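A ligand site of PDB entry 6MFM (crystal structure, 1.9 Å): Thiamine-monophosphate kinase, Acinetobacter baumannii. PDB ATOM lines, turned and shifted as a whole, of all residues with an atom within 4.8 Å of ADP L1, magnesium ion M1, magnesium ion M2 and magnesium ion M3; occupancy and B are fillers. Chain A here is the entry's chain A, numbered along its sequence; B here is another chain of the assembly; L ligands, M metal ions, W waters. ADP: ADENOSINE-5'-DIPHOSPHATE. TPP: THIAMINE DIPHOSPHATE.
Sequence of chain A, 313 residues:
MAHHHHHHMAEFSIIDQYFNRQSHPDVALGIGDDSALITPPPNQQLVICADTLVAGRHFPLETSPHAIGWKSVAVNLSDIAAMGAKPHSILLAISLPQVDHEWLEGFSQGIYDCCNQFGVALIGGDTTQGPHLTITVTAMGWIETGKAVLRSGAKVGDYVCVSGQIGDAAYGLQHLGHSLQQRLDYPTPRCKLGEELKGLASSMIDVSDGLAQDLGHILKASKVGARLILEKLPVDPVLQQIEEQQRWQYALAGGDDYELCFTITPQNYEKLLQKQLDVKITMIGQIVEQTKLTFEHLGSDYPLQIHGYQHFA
The nearest printed residue that does not touch magnesium ion M1 is Ala 50 of chain B (4.4 Å).
Merely in contact with magnesium ion M3: Arg 151 of chain B (3.7 Å). Of the 24 residues printed, 4 come within 4 Å of magnesium ion M3.
The backbone carbonyl oxygen of Leu 92 lies within hydrogen-bond range of the backbone NH of Asp 126 (2.9 Å). The backbone carbonyl oxygen (O) of Asp 126 lies within hydrogen-bond range of the backbone NH (N) of Ile 94 (2.9 Å). The side-chain carboxylate (OD2) of Asp 34 lies within salt-bridge range of the guanidinium group (NE) of Arg 151 of chain B, at 3.2 Å. The guanidinium group (NE) of Arg 151 of chain B lies within salt-bridge range of the side-chain carboxylate (OD1) of Asp 33 (3.9 Å). The backbone carbonyl oxygen (O) of Gly 124 lies within hydrogen-bond range of the backbone NH (N) of Leu 92 (2.9 Å). The side-chain carboxylate (OD1) of Asp 209 of chain B sits close to the side-chain hydroxyl (OG) of Ser 208 of chain B (3.4 Å).
Two residues have an atom within 4 Å of magnesium ion M2: Asp 51 of chain B and Asp 79 of chain B.
Magnesium ion M3 is bound by an oxygen (O1B) of ADP L1 (1.9 Å), the side-chain carboxylate (OD1) of Asp 79 of chain B (2.0 Å), the side-chain carboxylate (OD1) of Asp 206 of chain B (2.2 Å), water W14 (2.2 Å), water W10 (2.2 Å) and the side-chain carboxylate (OD1) of Asp 34 (2.2 Å). Magnesium ion M3 has six donor atoms within binding distance.
Magnesium ion M1 is bound by O1B of TPP L2. Magnesium ion M1 is bound by OD1 of Asp 51 of chain B (2.0 Å). The side-chain carboxylate (OD1) of Asp 126 binds magnesium ion M1 (2.2 Å). O2A of ADP L1 binds magnesium ion M1 (2.2 Å). Magnesium ion M1 is bound by water W6. O3B of ADP L1 binds magnesium ion M1, at 2.5 Å.
The backbone NH (N) of Asp 126 lies within hydrogen-bond range of a nitrogen (N7) of ADP L1 (3.1 Å). The backbone NH (N) of Asp 33 is in hydrogen-bond range of an oxygen (O3') of ADP L1. An oxygen (O3') of ADP L1 lies within hydrogen-bond range of the backbone carbonyl oxygen (O) of Asp 33, 2.6 Å away. The backbone NH of Gly 32 lies within hydrogen-bond range of an oxygen (O3') of ADP L1. N7 of ADP L1 sits at hydrogen-bond distance from N of Thr 127, 3.4 Å away. OG1 of Thr 127 sits at hydrogen-bond distance from N7 of ADP L1. N of Gly 125 lies within hydrogen-bond range of O2' of ADP L1, 3.0 Å away. An oxygen (O2') of ADP L1 lies close to the backbone carbonyl oxygen of Gly 125 (3.3 Å). The guanidinium group (NH2) of Arg 151 of chain B sits close to an oxygen (O1B) of ADP L1 (3.1 Å). An oxygen (O2B) of ADP L1 is in hydrogen-bond range of the side-chain hydroxyl (OG) of Ser 208 of chain B (3.4 Å). The backbone carbonyl oxygen (O) of Leu 92 sits at hydrogen-bond distance from a nitrogen (N6) of ADP L1, 3.5 Å away. OG of Ser 208 of chain B lies close to O3B of TPP L2 (2.9 Å).
The backbone carbonyl oxygen (O) of Gly 124 lies close to a nitrogen (N3) of ADP L1, 3.4 Å away. Glu 11 touches ADP L1 (OE2 to O2A, 3.8 Å). Phe 12 touches ADP L1 (CE1 to O1A, 3.9 Å). CD1 of Ile 15 touches C8 of ADP L1, 3.4 Å away. Phe 19 touches ADP L1. CG1 of Ile 31 touches N3 of ADP L1 (3.6 Å). Within 4 Å of ADP L1: Glu 11, Phe 12, Ile 15, Phe 19, Ile 31, Gly 32, Asp 33, Asp 34, Leu 92, Gly 124, Gly 125, Asp 126, Thr 127, Asp 51 of chain B, Asp 79 of chain B, Arg 151 of chain B and Ser 208 of chain B. Along chain A the residues within 4 Å of ADP L1 span positions 11 to 127. The nearest printed residue that does not touch ADP L1 is Ile 94 (4.1 Å).
Water W6 lies within hydrogen-bond range of the backbone carbonyl oxygen (O) of Gly 125 and an oxygen (O3A) of ADP L1. Water W10 lies within hydrogen-bond range of the backbone carbonyl oxygen (O) of Asp 206 of chain B (2.9 Å), an oxygen (O2B) of ADP L1 (3.1 Å), the side-chain hydroxyl (OG) of Ser 208 of chain B (3.4 Å) and the guanidinium group (NH2) of Arg 151 of chain B (3.4 Å). Water W13 lies within hydrogen-bond range of the backbone carbonyl oxygen (O) of Asp 34 (2.8 Å) and an oxygen (O3A) of ADP L1 (3.1 Å). Water W11 lies within hydrogen-bond range of OE2 of Glu 11, N of Thr 127 and O5' of ADP L1. Water W3 bridges OE2 of Glu 11 and O1A of ADP L1. Water W7 lies within hydrogen-bond range of N of Asp 33, O3' of ADP L1 and N of Gly 32.
Magnesium ion M2 is bound by O2B of TPP L2 (2.0 Å), OD2 of Asp 79 of chain B (2.1 Å), OD2 of Asp 51 of chain B (2.1 Å), O3B of ADP L1 (2.1 Å), water W14 (2.1 Å) and water W12 (2.2 Å). Magnesium ion M2 has six donor atoms within binding distance.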
ATOM      1  N   GLU A  11       6.496  -8.607 -16.583  1.00  0.00           N
ATOM      2  CA  GLU A  11       6.876  -9.824 -17.321  1.00  0.00           C
ATOM      3  C   GLU A  11       7.176 -10.996 -16.382  1.00  0.00           C
ATOM      4  O   GLU A  11       6.679 -12.108 -16.585  1.00  0.00           O
ATOM      5  CB  GLU A  11       8.091  -9.528 -18.194  1.00  0.00           C
ATOM      6  CG  GLU A  11       8.650 -10.772 -18.921  1.00  0.00           C
ATOM      7  CD  GLU A  11      10.070 -10.574 -19.399  1.00  0.00           C
ATOM      8  OE1 GLU A  11      10.580  -9.425 -19.317  1.00  0.00           O
ATOM      9  OE2 GLU A  11      10.696 -11.559 -19.848  1.00  0.00           O
ATOM     10  N   PHE A  12       8.022 -10.773 -15.380  1.00  0.00           N
ATOM     11  CA  PHE A  12       8.466 -11.894 -14.555  1.00  0.00           C
ATOM     12  C   PHE A  12       7.336 -12.441 -13.679  1.00  0.00           C
ATOM     13  O   PHE A  12       7.301 -13.646 -13.386  1.00  0.00           O
ATOM     14  CB  PHE A  12       9.658 -11.470 -13.698  1.00  0.00           C
ATOM     15  CG  PHE A  12      10.849 -11.041 -14.507  1.00  0.00           C
ATOM     16  CD1 PHE A  12      11.169 -11.699 -15.690  1.00  0.00           C
ATOM     17  CD2 PHE A  12      11.634  -9.972 -14.101  1.00  0.00           C
ATOM     18  CE1 PHE A  12      12.268 -11.301 -16.447  1.00  0.00           C
ATOM     19  CE2 PHE A  12      12.729  -9.565 -14.859  1.00  0.00           C
ATOM     20  CZ  PHE A  12      13.050 -10.233 -16.027  1.00  0.00           C
ATOM     21  N   ILE A  15       5.015 -14.851 -16.050  1.00  0.00           N
ATOM     22  CA  ILE A  15       5.521 -16.206 -16.221  1.00  0.00           C
ATOM     23  C   ILE A  15       5.261 -17.016 -14.950  1.00  0.00           C
ATOM     24  O   ILE A  15       4.707 -18.127 -15.000  1.00  0.00           O
ATOM     25  CB  ILE A  15       7.013 -16.168 -16.571  1.00  0.00           C
ATOM     26  CG1 ILE A  15       7.238 -15.305 -17.821  1.00  0.00           C
ATOM     27  CG2 ILE A  15       7.569 -17.573 -16.723  1.00  0.00           C
ATOM     28  CD1 ILE A  15       8.673 -14.863 -18.012  1.00  0.00           C
ATOM     29  N   PHE A  19       2.382 -19.443 -16.112  1.00  0.00           N
ATOM     30  CA  PHE A  19       2.996 -20.377 -17.043  1.00  0.00           C
ATOM     31  C   PHE A  19       4.059 -21.231 -16.383  1.00  0.00           C
ATOM     32  O   PHE A  19       4.976 -21.701 -17.061  1.00  0.00           O
ATOM     33  CB  PHE A  19       3.601 -19.633 -18.242  1.00  0.00           C
ATOM     34  CG  PHE A  19       2.610 -18.786 -18.988  1.00  0.00           C
ATOM     35  CD1 PHE A  19       1.538 -19.368 -19.634  1.00  0.00           C
ATOM     36  CD2 PHE A  19       2.751 -17.409 -19.036  1.00  0.00           C
ATOM     37  CE1 PHE A  19       0.627 -18.607 -20.323  1.00  0.00           C
ATOM     38  CE2 PHE A  19       1.834 -16.628 -19.719  1.00  0.00           C
ATOM     39  CZ  PHE A  19       0.768 -17.230 -20.371  1.00  0.00           C
ATOM     40  N   ILE A  31      11.074 -24.615 -16.970  1.00  0.00           N
ATOM     41  CA  ILE A  31      11.102 -23.160 -16.929  1.00  0.00           C
ATOM     42  C   ILE A  31      11.996 -22.631 -15.807  1.00  0.00           C
ATOM     43  O   ILE A  31      11.940 -23.096 -14.665  1.00  0.00           O
ATOM     44  CB  ILE A  31       9.659 -22.649 -16.775  1.00  0.00           C
ATOM     45  CG1 ILE A  31       8.886 -22.953 -18.064  1.00  0.00           C
ATOM     46  CG2 ILE A  31       9.616 -21.176 -16.410  1.00  0.00           C
ATOM     47  CD1 ILE A  31       7.400 -23.115 -17.883  1.00  0.00           C
ATOM     48  N   GLY A  32      12.823 -21.622 -16.144  1.00  0.00           N
ATOM     49  CA  GLY A  32      13.549 -20.856 -15.144  1.00  0.00           C
ATOM     50  C   GLY A  32      14.997 -20.567 -15.495  1.00  0.00           C
ATOM     51  O   GLY A  32      15.658 -19.789 -14.806  1.00  0.00           O
ATOM     52  N   ASP A  33      15.517 -21.223 -16.532  1.00  0.00           N
ATOM     53  CA  ASP A  33      16.899 -21.028 -16.975  1.00  0.00           C
ATOM     54  C   ASP A  33      16.879 -20.472 -18.397  1.00  0.00           C
ATOM     55  O   ASP A  33      15.808 -20.253 -18.980  1.00  0.00           O
ATOM     56  CB  ASP A  33      17.687 -22.344 -16.903  1.00  0.00           C
ATOM     57  CG  ASP A  33      19.130 -22.135 -16.420  1.00  0.00           C
ATOM     58  OD1 ASP A  33      19.899 -21.476 -17.146  1.00  0.00           O
ATOM     59  OD2 ASP A  33      19.495 -22.628 -15.314  1.00  0.00           O
ATOM     60  N   ASP A  34      18.070 -20.273 -18.969  1.00  0.00           N
ATOM     61  CA  ASP A  34      18.158 -19.716 -20.316  1.00  0.00           C
ATOM     62  C   ASP A  34      17.574 -20.653 -21.368  1.00  0.00           C
ATOM     63  O   ASP A  34      16.967 -20.178 -22.332  1.00  0.00           O
ATOM     64  CB  ASP A  34      19.620 -19.366 -20.614  1.00  0.00           C
ATOM     65  CG  ASP A  34      20.167 -18.397 -19.593  1.00  0.00           C
ATOM     66  OD1 ASP A  34      19.885 -17.180 -19.717  1.00  0.00           O
ATOM     67  OD2 ASP A  34      20.795 -18.870 -18.617  1.00  0.00           O
ATOM     68  N   LEU A  92       6.246 -21.771 -25.428  1.00  0.00           N
ATOM     69  CA  LEU A  92       5.203 -20.776 -25.658  1.00  0.00           C
ATOM     70  C   LEU A  92       5.815 -19.380 -25.754  1.00  0.00           C
ATOM     71  O   LEU A  92       6.355 -18.866 -24.761  1.00  0.00           O
ATOM     72  CB  LEU A  92       4.159 -20.816 -24.527  1.00  0.00           C
ATOM     73  CG  LEU A  92       3.118 -19.695 -24.521  1.00  0.00           C
ATOM     74  CD1 LEU A  92       2.304 -19.711 -25.803  1.00  0.00           C
ATOM     75  CD2 LEU A  92       2.198 -19.789 -23.275  1.00  0.00           C
ATOM     76  N   ILE A  94       4.721 -15.537 -26.491  1.00  0.00           N
ATOM     77  CA  ILE A  94       3.543 -14.692 -26.618  1.00  0.00           C
ATOM     78  C   ILE A  94       3.975 -13.228 -26.596  1.00  0.00           C
ATOM     79  O   ILE A  94       4.749 -12.812 -25.737  1.00  0.00           O
ATOM     80  CB  ILE A  94       2.488 -14.985 -25.528  1.00  0.00           C
ATOM     81  CG1 ILE A  94       1.295 -14.049 -25.675  1.00  0.00           C
ATOM     82  CG2 ILE A  94       3.101 -14.878 -24.126  1.00  0.00           C
ATOM     83  CD1 ILE A  94       0.010 -14.562 -25.022  1.00  0.00           C
ATOM     84  N   LEU A 122       4.602 -27.989 -20.765  1.00  0.00           N
ATOM     85  CA  LEU A 122       5.051 -26.657 -21.172  1.00  0.00           C
ATOM     86  C   LEU A 122       6.372 -26.389 -20.463  1.00  0.00           C
ATOM     87  O   LEU A 122       6.409 -26.253 -19.234  1.00  0.00           O
ATOM     88  CB  LEU A 122       4.009 -25.594 -20.846  1.00  0.00           C
ATOM     89  CG  LEU A 122       4.408 -24.113 -20.984  1.00  0.00           C
ATOM     90  CD1 LEU A 122       4.810 -23.790 -22.437  1.00  0.00           C
ATOM     91  CD2 LEU A 122       3.264 -23.224 -20.525  1.00  0.00           C
ATOM     92  N   GLY A 124       9.004 -24.069 -21.456  1.00  0.00           N
ATOM     93  CA  GLY A 124       9.698 -22.808 -21.610  1.00  0.00           C
ATOM     94  C   GLY A 124       8.996 -21.921 -22.618  1.00  0.00           C
ATOM     95  O   GLY A 124       7.907 -22.226 -23.107  1.00  0.00           O
ATOM     96  N   GLY A 125       9.625 -20.797 -22.922  1.00  0.00           N
ATOM     97  CA  GLY A 125       9.076 -19.881 -23.903  1.00  0.00           C
ATOM     98  C   GLY A 125       9.600 -18.464 -23.679  1.00  0.00           C
ATOM     99  O   GLY A 125      10.722 -18.273 -23.231  1.00  0.00           O
ATOM    100  N   ASP A 126       8.748 -17.493 -24.004  1.00  0.00           N
ATOM    101  CA  ASP A 126       9.160 -16.096 -23.978  1.00  0.00           C
ATOM    102  C   ASP A 126       7.907 -15.224 -23.942  1.00  0.00           C
ATOM    103  O   ASP A 126       6.938 -15.484 -24.651  1.00  0.00           O
ATOM    104  CB  ASP A 126      10.051 -15.737 -25.179  1.00  0.00           C
ATOM    105  CG  ASP A 126      10.805 -14.417 -24.988  1.00  0.00           C
ATOM    106  OD1 ASP A 126      11.434 -14.213 -23.932  1.00  0.00           O
ATOM    107  OD2 ASP A 126      10.793 -13.568 -25.907  1.00  0.00           O
ATOM    108  N   THR A 127       7.953 -14.196 -23.098  1.00  0.00           N
ATOM    109  CA  THR A 127       6.851 -13.266 -22.913  1.00  0.00           C
ATOM    110  C   THR A 127       7.355 -11.870 -23.243  1.00  0.00           C
ATOM    111  O   THR A 127       8.333 -11.414 -22.637  1.00  0.00           O
ATOM    112  CB  THR A 127       6.363 -13.325 -21.455  1.00  0.00           C
ATOM    113  OG1 THR A 127       6.058 -14.681 -21.118  1.00  0.00           O
ATOM    114  CG2 THR A 127       5.134 -12.451 -21.261  1.00  0.00           C
ATOM    115  N   ALA B  50      13.503 -20.218 -26.904  1.00  0.00           N
ATOM    116  CA  ALA B  50      12.909 -19.368 -27.931  1.00  0.00           C
ATOM    117  C   ALA B  50      12.727 -17.958 -27.399  1.00  0.00           C
ATOM    118  O   ALA B  50      12.334 -17.755 -26.245  1.00  0.00           O
ATOM    119  CB  ALA B  50      11.562 -19.937 -28.407  1.00  0.00           C
ATOM    120  N   ASP B  51      13.007 -16.975 -28.256  1.00  0.00           N
ATOM    121  CA  ASP B  51      12.977 -15.544 -27.916  1.00  0.00           C
ATOM    122  C   ASP B  51      12.334 -14.807 -29.074  1.00  0.00           C
ATOM    123  O   ASP B  51      12.649 -15.088 -30.237  1.00  0.00           O
ATOM    124  CB  ASP B  51      14.377 -14.960 -27.697  1.00  0.00           C
ATOM    125  CG  ASP B  51      14.835 -14.984 -26.225  1.00  0.00           C
ATOM    126  OD1 ASP B  51      14.000 -15.173 -25.327  1.00  0.00           O
ATOM    127  OD2 ASP B  51      16.042 -14.777 -25.990  1.00  0.00           O
ATOM    128  N   VAL B  75      20.566 -13.658 -30.579  1.00  0.00           N
ATOM    129  CA  VAL B  75      20.125 -13.619 -29.178  1.00  0.00           C
ATOM    130  C   VAL B  75      19.726 -15.019 -28.709  1.00  0.00           C
ATOM    131  O   VAL B  75      19.836 -15.342 -27.526  1.00  0.00           O
ATOM    132  CB  VAL B  75      18.995 -12.596 -28.958  1.00  0.00           C
ATOM    133  CG1 VAL B  75      19.399 -11.225 -29.491  1.00  0.00           C
ATOM    134  CG2 VAL B  75      17.703 -13.026 -29.635  1.00  0.00           C
ATOM    135  N   ASP B  79      21.414 -17.782 -25.704  1.00  0.00           N
ATOM    136  CA  ASP B  79      20.771 -18.529 -24.629  1.00  0.00           C
ATOM    137  C   ASP B  79      21.196 -19.991 -24.598  1.00  0.00           C
ATOM    138  O   ASP B  79      21.140 -20.629 -23.539  1.00  0.00           O
ATOM    139  CB  ASP B  79      19.250 -18.432 -24.751  1.00  0.00           C
ATOM    140  CG  ASP B  79      18.682 -17.274 -23.946  1.00  0.00           C
ATOM    141  OD1 ASP B  79      19.131 -17.087 -22.806  1.00  0.00           O
ATOM    142  OD2 ASP B  79      17.800 -16.550 -24.439  1.00  0.00           O
ATOM    143  N   ARG B 151      21.798 -21.610 -13.715  1.00  0.00           N
ATOM    144  CA  ARG B 151      21.810 -20.333 -13.000  1.00  0.00           C
ATOM    145  C   ARG B 151      21.941 -20.531 -11.503  1.00  0.00           C
ATOM    146  O   ARG B 151      22.301 -19.583 -10.798  1.00  0.00           O
ATOM    147  CB  ARG B 151      20.540 -19.527 -13.292  1.00  0.00           C
ATOM    148  CG  ARG B 151      20.422 -18.980 -14.728  1.00  0.00           C
ATOM    149  CD  ARG B 151      19.122 -18.221 -14.909  1.00  0.00           C
ATOM    150  NE  ARG B 151      18.906 -17.755 -16.293  1.00  0.00           N
ATOM    151  CZ  ARG B 151      17.903 -16.949 -16.634  1.00  0.00           C
ATOM    152  NH1 ARG B 151      17.040 -16.531 -15.719  1.00  0.00           N
ATOM    153  NH2 ARG B 151      17.758 -16.552 -17.892  1.00  0.00           N
ATOM    154  N   ILE B 205      24.822 -17.034 -17.043  1.00  0.00           N
ATOM    155  CA  ILE B 205      23.623 -16.440 -17.648  1.00  0.00           C
ATOM    156  C   ILE B 205      24.105 -15.536 -18.777  1.00  0.00           C
ATOM    157  O   ILE B 205      25.226 -15.035 -18.734  1.00  0.00           O
ATOM    158  CB  ILE B 205      22.781 -15.672 -16.605  1.00  0.00           C
ATOM    159  CG1 ILE B 205      21.420 -15.241 -17.170  1.00  0.00           C
ATOM    160  CG2 ILE B 205      23.562 -14.438 -16.073  1.00  0.00           C
ATOM    161  CD1 ILE B 205      20.440 -14.795 -16.093  1.00  0.00           C
ATOM    162  N   ASP B 206      23.280 -15.325 -19.798  1.00  0.00           N
ATOM    163  CA  ASP B 206      23.685 -14.339 -20.787  1.00  0.00           C
ATOM    164  C   ASP B 206      23.062 -12.989 -20.439  1.00  0.00           C
ATOM    165  O   ASP B 206      21.922 -12.930 -19.947  1.00  0.00           O
ATOM    166  CB  ASP B 206      23.378 -14.734 -22.230  1.00  0.00           C
ATOM    167  CG  ASP B 206      21.916 -14.844 -22.502  1.00  0.00           C
ATOM    168  OD1 ASP B 206      21.220 -15.371 -21.617  1.00  0.00           O
ATOM    169  OD2 ASP B 206      21.477 -14.424 -23.608  1.00  0.00           O
ATOM    170  N   SER B 208      21.261 -10.244 -21.280  1.00  0.00           N
ATOM    171  CA  SER B 208      20.301  -9.659 -22.209  1.00  0.00           C
ATOM    172  C   SER B 208      19.536  -8.487 -21.606  1.00  0.00           C
ATOM    173  O   SER B 208      19.224  -7.532 -22.333  1.00  0.00           O
ATOM    174  CB  SER B 208      19.312 -10.722 -22.689  1.00  0.00           C
ATOM    175  OG  SER B 208      18.703 -11.403 -21.600  1.00  0.00           O
ATOM    176  N   ASP B 209      19.263  -8.507 -20.297  1.00  0.00           N
ATOM    177  CA  ASP B 209      18.519  -7.452 -19.630  1.00  0.00           C
ATOM    178  C   ASP B 209      19.404  -6.353 -19.072  1.00  0.00           C
ATOM    179  O   ASP B 209      18.958  -5.214 -18.948  1.00  0.00           O
ATOM    180  CB  ASP B 209      17.712  -8.010 -18.450  1.00  0.00           C
ATOM    181  CG  ASP B 209      16.694  -9.033 -18.857  1.00  0.00           C
ATOM    182  OD1 ASP B 209      16.521  -9.253 -20.072  1.00  0.00           O
ATOM    183  OD2 ASP B 209      16.071  -9.618 -17.926  1.00  0.00           O
HETATM  184  PB  ADP L   1      16.118 -15.148 -21.205  1.00  0.00           P
HETATM  185  O1B ADP L   1      17.250 -16.140 -20.890  1.00  0.00           O
HETATM  186  O2B ADP L   1      16.421 -13.745 -20.718  1.00  0.00           O
HETATM  187  O3B ADP L   1      15.791 -15.228 -22.704  1.00  0.00           O
HETATM  188  PA  ADP L   1      13.432 -14.938 -20.111  1.00  0.00           P
HETATM  189  O1A ADP L   1      13.655 -13.930 -18.953  1.00  0.00           O
HETATM  190  O2A ADP L   1      12.928 -14.285 -21.345  1.00  0.00           O
HETATM  191  O3A ADP L   1      14.827 -15.657 -20.417  1.00  0.00           O
HETATM  192  O5' ADP L   1      12.476 -16.086 -19.532  1.00  0.00           O
HETATM  193  C5' ADP L   1      12.786 -16.652 -18.241  1.00  0.00           C
HETATM  194  C4' ADP L   1      12.320 -18.081 -18.199  1.00  0.00           C
HETATM  195  O4' ADP L   1      10.881 -18.132 -18.387  1.00  0.00           O
HETATM  196  C3' ADP L   1      12.937 -19.006 -19.245  1.00  0.00           C
HETATM  197  O3' ADP L   1      13.205 -20.251 -18.624  1.00  0.00           O
HETATM  198  C2' ADP L   1      11.836 -19.102 -20.321  1.00  0.00           C
HETATM  199  O2' ADP L   1      11.913 -20.353 -21.024  1.00  0.00           O
HETATM  200  C1' ADP L   1      10.568 -18.994 -19.475  1.00  0.00           C
HETATM  201  N9  ADP L   1       9.403 -18.428 -20.159  1.00  0.00           N
HETATM  202  C8  ADP L   1       9.260 -17.115 -20.537  1.00  0.00           C
HETATM  203  N7  ADP L   1       8.065 -16.821 -21.011  1.00  0.00           N
HETATM  204  C5  ADP L   1       7.389 -18.030 -20.963  1.00  0.00           C
HETATM  205  C6  ADP L   1       6.076 -18.402 -21.312  1.00  0.00           C
HETATM  206  N6  ADP L   1       5.147 -17.538 -21.768  1.00  0.00           N
HETATM  207  N1  ADP L   1       5.710 -19.690 -21.142  1.00  0.00           N
HETATM  208  C2  ADP L   1       6.610 -20.551 -20.634  1.00  0.00           C
HETATM  209  N3  ADP L   1       7.871 -20.317 -20.257  1.00  0.00           N
HETATM  210  C4  ADP L   1       8.200 -19.030 -20.443  1.00  0.00           C
HETATM  211  N1' TPP L   2      14.359   0.135 -27.682  1.00  0.00           N
HETATM  212  C2' TPP L   2      14.773  -0.238 -28.908  1.00  0.00           C
HETATM  213  CM2 TPP L   2      14.130   0.429 -30.072  1.00  0.00           C
HETATM  214  N3' TPP L   2      15.713  -1.151 -29.158  1.00  0.00           N
HETATM  215  C4' TPP L   2      16.294  -1.766 -28.118  1.00  0.00           C
HETATM  216  N4' TPP L   2      17.203  -2.700 -28.404  1.00  0.00           N
HETATM  217  C5' TPP L   2      15.928  -1.431 -26.779  1.00  0.00           C
HETATM  218  C6' TPP L   2      14.948  -0.477 -26.647  1.00  0.00           C
HETATM  219  C7' TPP L   2      16.576  -2.079 -25.578  1.00  0.00           C
HETATM  220  N3  TPP L   2      16.026  -3.425 -25.281  1.00  0.00           N
HETATM  221  C2  TPP L   2      15.053  -3.992 -25.964  1.00  0.00           C
HETATM  222  S1  TPP L   2      14.706  -5.538 -25.422  1.00  0.00           S
HETATM  223  C5  TPP L   2      15.929  -5.421 -24.189  1.00  0.00           C
HETATM  224  C4  TPP L   2      16.535  -4.217 -24.246  1.00  0.00           C
HETATM  225  CM4 TPP L   2      17.617  -3.711 -23.364  1.00  0.00           C
HETATM  226  C6  TPP L   2      16.230  -6.573 -23.272  1.00  0.00           C
HETATM  227  C7  TPP L   2      16.467  -7.803 -24.121  1.00  0.00           C
HETATM  228  O7  TPP L   2      15.193  -8.228 -24.663  1.00  0.00           O
HETATM  229  PA  TPP L   2      14.275  -9.347 -23.946  1.00  0.00           P
HETATM  230  O1A TPP L   2      14.167  -9.118 -22.482  1.00  0.00           O
HETATM  231  O2A TPP L   2      12.968  -9.505 -24.588  1.00  0.00           O
HETATM  232  O3A TPP L   2      15.166 -10.632 -24.213  1.00  0.00           O
HETATM  233  PB  TPP L   2      15.440 -11.945 -23.357  1.00  0.00           P
HETATM  234  O1B TPP L   2      14.134 -12.741 -23.486  1.00  0.00           O
HETATM  235  O2B TPP L   2      16.617 -12.610 -24.067  1.00  0.00           O
HETATM  236  O3B TPP L   2      15.796 -11.548 -21.917  1.00  0.00           O
HETATM  237 MG    MG M   1      13.505 -14.632 -23.420  1.00  0.00          MG
HETATM  238 MG    MG M   2      17.179 -14.571 -24.198  1.00  0.00          MG
HETATM  239 MG    MG M   3      19.125 -15.773 -21.277  1.00  0.00          MG
HETATM  240 MG    MG M   4      14.589 -10.231 -20.865  1.00  0.00          MG
HETATM  241  O   HOH W   1      13.459 -22.454 -23.006  1.00  0.00           O
HETATM  242  O   HOH W   2      15.729 -14.419 -17.322  1.00  0.00           O
HETATM  243  O   HOH W   3      12.775 -11.535 -21.176  1.00  0.00           O
HETATM  244  O   HOH W   4      17.775 -12.508 -18.472  1.00  0.00           O
HETATM  245  O   HOH W   5      13.155 -19.861 -24.019  1.00  0.00           O
HETATM  246  O   HOH W   6      13.076 -16.744 -22.913  1.00  0.00           O
HETATM  247  O   HOH W   7      14.705 -23.196 -18.446  1.00  0.00           O
HETATM  248  O   HOH W   8      14.997 -11.676 -18.948  1.00  0.00           O
HETATM  249  O   HOH W   9      12.943 -22.747 -20.427  1.00  0.00           O
HETATM  250  O   HOH W  10      19.320 -14.172 -19.789  1.00  0.00           O
HETATM  251  O   HOH W  11      10.260 -13.927 -21.134  1.00  0.00           O
HETATM  252  O   HOH W  12      18.738 -13.871 -25.562  1.00  0.00           O
HETATM  253  O   HOH W  13      15.537 -17.791 -22.584  1.00  0.00           O
HETATM  254  O   HOH W  14      18.649 -14.178 -22.684  1.00  0.00           O
